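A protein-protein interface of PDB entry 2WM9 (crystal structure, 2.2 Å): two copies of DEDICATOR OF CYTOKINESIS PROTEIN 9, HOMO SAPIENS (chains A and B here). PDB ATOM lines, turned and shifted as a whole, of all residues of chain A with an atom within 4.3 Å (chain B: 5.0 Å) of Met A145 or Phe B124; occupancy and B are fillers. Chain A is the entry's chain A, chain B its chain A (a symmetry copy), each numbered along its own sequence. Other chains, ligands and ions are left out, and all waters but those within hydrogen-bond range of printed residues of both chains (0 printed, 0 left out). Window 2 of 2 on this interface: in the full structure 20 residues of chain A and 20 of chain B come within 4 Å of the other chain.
Tyr A138 touches Phe B124 (CB to O, 3.6 Å). Leu B127 touches Tyr A138 (CD1 to CE1, 3.9 Å). Ala B128 touches Tyr A138. Phe B124 touches Val A141. Thr A142 touches Phe B124 (CG2 to CB, 3.9 Å). Thr A142 touches Glu B125 (CG2 to N, 3.8 Å). Met A145 touches Phe B124 (SD to CD2, 3.6 Å).
Printed residues of chain B within 4 Å of Met A145: Phe B124. Printed residues of chain A within 4 Å of Phe B124: Tyr A138, Val A141, Thr A142 and Met A145. Of the printed residues of chain A, Ala B128 touches Tyr A138 (3.7 Å). Of the printed residues of chain B, Thr A142 touches Phe B124 and Glu B125. Arg B126 touches none of the printed residues of chain A. The nearest printed residue of chain A that does not touch Phe B124 is Glu A143 (7.6 Å). The nearest printed residue of chain B that does not touch Val A141 is Glu B125 (6.9 Å).
Of the 8 printed residues of chain A, 4 touch a printed residue of chain B. Printed residues of chain A that touch a printed residue of chain B: Tyr A138, Val A141, Thr A142 and Met A145. Hydrophobic or aromatic side chains of chain A that line the printed part of chain B: Tyr A138, Val A141 and Met A145.
No position is printed for both chains.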
ATOM      1  N   TYR A 138      -2.605 -10.496  -7.247  1.00  0.00           N
ATOM      2  CA  TYR A 138      -3.484 -11.488  -7.871  1.00  0.00           C
ATOM      3  C   TYR A 138      -4.503 -10.880  -8.831  1.00  0.00           C
ATOM      4  O   TYR A 138      -4.850 -11.505  -9.843  1.00  0.00           O
ATOM      5  CB  TYR A 138      -4.110 -12.456  -6.839  1.00  0.00           C
ATOM      6  CG  TYR A 138      -3.028 -13.353  -6.308  1.00  0.00           C
ATOM      7  CD1 TYR A 138      -2.547 -14.414  -7.077  1.00  0.00           C
ATOM      8  CD2 TYR A 138      -2.416 -13.093  -5.072  1.00  0.00           C
ATOM      9  CE1 TYR A 138      -1.542 -15.215  -6.623  1.00  0.00           C
ATOM     10  CE2 TYR A 138      -1.407 -13.862  -4.618  1.00  0.00           C
ATOM     11  CZ  TYR A 138      -0.971 -14.936  -5.389  1.00  0.00           C
ATOM     12  OH  TYR A 138       0.058 -15.722  -4.922  1.00  0.00           O
ATOM     13  N   VAL A 141      -2.537 -10.450 -11.881  1.00  0.00           N
ATOM     14  CA  VAL A 141      -2.312 -11.750 -12.498  1.00  0.00           C
ATOM     15  C   VAL A 141      -3.470 -12.150 -13.419  1.00  0.00           C
ATOM     16  O   VAL A 141      -3.247 -12.516 -14.575  1.00  0.00           O
ATOM     17  CB  VAL A 141      -2.028 -12.858 -11.462  1.00  0.00           C
ATOM     18  CG1 VAL A 141      -2.129 -14.207 -12.096  1.00  0.00           C
ATOM     19  CG2 VAL A 141      -0.636 -12.657 -10.860  1.00  0.00           C
ATOM     20  N   THR A 142      -4.705 -12.088 -12.920  1.00  0.00           N
ATOM     21  CA  THR A 142      -5.854 -12.426 -13.757  1.00  0.00           C
ATOM     22  C   THR A 142      -5.966 -11.415 -14.921  1.00  0.00           C
ATOM     23  O   THR A 142      -6.307 -11.761 -16.032  1.00  0.00           O
ATOM     24  CB  THR A 142      -7.173 -12.437 -12.973  1.00  0.00           C
ATOM     25  OG1 THR A 142      -7.379 -11.146 -12.355  1.00  0.00           O
ATOM     26  CG2 THR A 142      -7.175 -13.545 -11.925  1.00  0.00           C
ATOM     27  N   GLU A 143      -5.653 -10.164 -14.653  1.00  0.00           N
ATOM     28  CA  GLU A 143      -5.731  -9.139 -15.675  1.00  0.00           C
ATOM     29  C   GLU A 143      -4.766  -9.489 -16.846  1.00  0.00           C
ATOM     30  O   GLU A 143      -5.219  -9.800 -17.951  1.00  0.00           O
ATOM     31  CB  GLU A 143      -5.473  -7.764 -15.038  1.00  0.00           C
ATOM     32  CG  GLU A 143      -5.420  -6.582 -16.017  1.00  0.00           C
ATOM     33  CD  GLU A 143      -4.697  -5.356 -15.428  1.00  0.00           C
ATOM     34  OE1 GLU A 143      -3.676  -4.927 -16.012  1.00  0.00           O
ATOM     35  OE2 GLU A 143      -5.130  -4.837 -14.372  1.00  0.00           O
ATOM     36  N   VAL A 144      -3.457  -9.523 -16.580  1.00  0.00           N
ATOM     37  CA  VAL A 144      -2.460  -9.842 -17.616  1.00  0.00           C
ATOM     38  C   VAL A 144      -2.612 -11.268 -18.187  1.00  0.00           C
ATOM     39  O   VAL A 144      -2.385 -11.496 -19.368  1.00  0.00           O
ATOM     40  CB  VAL A 144      -0.985  -9.575 -17.150  1.00  0.00           C
ATOM     41  CG1 VAL A 144      -0.865  -8.211 -16.445  1.00  0.00           C
ATOM     42  CG2 VAL A 144      -0.483 -10.710 -16.281  1.00  0.00           C
ATOM     43  N   MET A 145      -3.034 -12.235 -17.383  1.00  0.00           N
ATOM     44  CA  MET A 145      -3.361 -13.540 -17.978  1.00  0.00           C
ATOM     45  C   MET A 145      -4.421 -13.424 -19.068  1.00  0.00           C
ATOM     46  O   MET A 145      -4.434 -14.222 -20.018  1.00  0.00           O
ATOM     47  CB  MET A 145      -3.829 -14.556 -16.948  1.00  0.00           C
ATOM     48  CG  MET A 145      -2.691 -15.224 -16.226  1.00  0.00           C
ATOM     49  SD  MET A 145      -3.267 -16.298 -14.920  1.00  0.00           S
ATOM     50  CE  MET A 145      -3.936 -17.666 -15.877  1.00  0.00           C
ATOM     51  N   HIS A 146      -5.317 -12.445 -18.934  1.00  0.00           N
ATOM     52  CA  HIS A 146      -6.327 -12.238 -19.966  1.00  0.00           C
ATOM     53  C   HIS A 146      -5.855 -11.340 -21.130  1.00  0.00           C
ATOM     54  O   HIS A 146      -6.087 -11.659 -22.295  1.00  0.00           O
ATOM     55  CB  HIS A 146      -7.625 -11.714 -19.356  1.00  0.00           C
ATOM     56  CG  HIS A 146      -8.619 -11.256 -20.374  1.00  0.00           C
ATOM     57  ND1 HIS A 146      -9.326 -12.136 -21.172  1.00  0.00           N
ATOM     58  CD2 HIS A 146      -9.015 -10.015 -20.738  1.00  0.00           C
ATOM     59  CE1 HIS A 146     -10.121 -11.453 -21.977  1.00  0.00           C
ATOM     60  NE2 HIS A 146      -9.959 -10.164 -21.729  1.00  0.00           N
ATOM     61  N   SER A 147      -5.178 -10.243 -20.812  1.00  0.00           N
ATOM     62  CA  SER A 147      -4.783  -9.265 -21.814  1.00  0.00           C
ATOM     63  C   SER A 147      -3.429  -9.465 -22.534  1.00  0.00           C
ATOM     64  O   SER A 147      -3.134  -8.755 -23.504  1.00  0.00           O
ATOM     65  CB  SER A 147      -4.739  -7.896 -21.172  1.00  0.00           C
ATOM     66  OG  SER A 147      -3.555  -7.776 -20.419  1.00  0.00           O
ATOM     67  N   ARG B 122      -3.966 -23.107  -9.107  1.00  0.00           N
ATOM     68  CA  ARG B 122      -3.804 -21.821  -9.805  1.00  0.00           C
ATOM     69  C   ARG B 122      -5.056 -20.943  -9.779  1.00  0.00           C
ATOM     70  O   ARG B 122      -5.365 -20.274 -10.758  1.00  0.00           O
ATOM     71  CB  ARG B 122      -3.322 -22.001 -11.275  1.00  0.00           C
ATOM     72  CG  ARG B 122      -2.344 -23.164 -11.580  1.00  0.00           C
ATOM     73  CD  ARG B 122      -1.269 -23.408 -10.554  1.00  0.00           C
ATOM     74  NE  ARG B 122      -0.031 -23.966 -11.126  1.00  0.00           N
ATOM     75  CZ  ARG B 122       0.515 -25.140 -10.792  1.00  0.00           C
ATOM     76  NH1 ARG B 122       1.648 -25.509 -11.353  1.00  0.00           N
ATOM     77  NH2 ARG B 122      -0.053 -25.956  -9.893  1.00  0.00           N
ATOM     78  N   ASP B 123      -5.817 -20.959  -8.690  1.00  0.00           N
ATOM     79  CA  ASP B 123      -7.062 -20.192  -8.711  1.00  0.00           C
ATOM     80  C   ASP B 123      -6.759 -18.798  -8.232  1.00  0.00           C
ATOM     81  O   ASP B 123      -6.909 -18.493  -7.037  1.00  0.00           O
ATOM     82  CB  ASP B 123      -8.153 -20.829  -7.849  1.00  0.00           C
ATOM     83  CG  ASP B 123      -9.516 -20.239  -8.130  1.00  0.00           C
ATOM     84  OD1 ASP B 123      -9.597 -19.088  -8.640  1.00  0.00           O
ATOM     85  OD2 ASP B 123     -10.514 -20.944  -7.871  1.00  0.00           O
ATOM     86  N   PHE B 124      -6.331 -17.954  -9.165  1.00  0.00           N
ATOM     87  CA  PHE B 124      -5.862 -16.616  -8.849  1.00  0.00           C
ATOM     88  C   PHE B 124      -6.976 -15.635  -8.509  1.00  0.00           C
ATOM     89  O   PHE B 124      -6.770 -14.712  -7.732  1.00  0.00           O
ATOM     90  CB  PHE B 124      -4.979 -16.069  -9.993  1.00  0.00           C
ATOM     91  CG  PHE B 124      -3.829 -16.965 -10.328  1.00  0.00           C
ATOM     92  CD1 PHE B 124      -2.855 -17.241  -9.379  1.00  0.00           C
ATOM     93  CD2 PHE B 124      -3.740 -17.570 -11.573  1.00  0.00           C
ATOM     94  CE1 PHE B 124      -1.789 -18.087  -9.675  1.00  0.00           C
ATOM     95  CE2 PHE B 124      -2.678 -18.407 -11.880  1.00  0.00           C
ATOM     96  CZ  PHE B 124      -1.691 -18.661 -10.937  1.00  0.00           C
ATOM     97  N   GLU B 125      -8.160 -15.840  -9.067  1.00  0.00           N
ATOM     98  CA  GLU B 125      -9.276 -14.983  -8.704  1.00  0.00           C
ATOM     99  C   GLU B 125      -9.693 -15.219  -7.231  1.00  0.00           C
ATOM    100  O   GLU B 125     -10.002 -14.255  -6.517  1.00  0.00           O
ATOM    101  CB  GLU B 125     -10.456 -15.156  -9.675  1.00  0.00           C
ATOM    102  CG  GLU B 125     -11.597 -14.157  -9.448  1.00  0.00           C
ATOM    103  CD  GLU B 125     -12.513 -14.575  -8.281  1.00  0.00           C
ATOM    104  OE1 GLU B 125     -12.654 -15.810  -8.066  1.00  0.00           O
ATOM    105  OE2 GLU B 125     -13.079 -13.683  -7.573  1.00  0.00           O
ATOM    106  N   ARG B 126      -9.670 -16.474  -6.775  1.00  0.00           N
ATOM    107  CA  ARG B 126      -9.990 -16.785  -5.369  1.00  0.00           C
ATOM    108  C   ARG B 126      -8.914 -16.261  -4.418  1.00  0.00           C
ATOM    109  O   ARG B 126      -9.217 -15.799  -3.324  1.00  0.00           O
ATOM    110  CB  ARG B 126     -10.116 -18.283  -5.144  1.00  0.00           C
ATOM    111  CG  ARG B 126     -11.240 -18.931  -5.896  1.00  0.00           C
ATOM    112  CD  ARG B 126     -12.559 -18.510  -5.392  1.00  0.00           C
ATOM    113  NE  ARG B 126     -13.383 -19.678  -5.077  1.00  0.00           N
ATOM    114  CZ  ARG B 126     -14.065 -20.402  -5.971  1.00  0.00           C
ATOM    115  NH1 ARG B 126     -13.997 -20.118  -7.270  1.00  0.00           N
ATOM    116  NH2 ARG B 126     -14.809 -21.436  -5.572  1.00  0.00           N
ATOM    117  N   LEU B 127      -7.651 -16.363  -4.833  1.00  0.00           N
ATOM    118  CA  LEU B 127      -6.579 -15.788  -4.051  1.00  0.00           C
ATOM    119  C   LEU B 127      -6.819 -14.278  -3.954  1.00  0.00           C
ATOM    120  O   LEU B 127      -6.750 -13.711  -2.863  1.00  0.00           O
ATOM    121  CB  LEU B 127      -5.197 -16.139  -4.652  1.00  0.00           C
ATOM    122  CG  LEU B 127      -4.805 -17.595  -4.360  1.00  0.00           C
ATOM    123  CD1 LEU B 127      -3.697 -18.127  -5.272  1.00  0.00           C
ATOM    124  CD2 LEU B 127      -4.424 -17.793  -2.887  1.00  0.00           C
ATOM    125  N   ALA B 128      -7.101 -13.617  -5.087  1.00  0.00           N
ATOM    126  CA  ALA B 128      -7.344 -12.176  -5.064  1.00  0.00           C
ATOM    127  C   ALA B 128      -8.457 -11.816  -4.063  1.00  0.00           C
ATOM    128  O   ALA B 128      -8.360 -10.825  -3.343  1.00  0.00           O
ATOM    129  CB  ALA B 128      -7.731 -11.639  -6.480  1.00  0.00           C
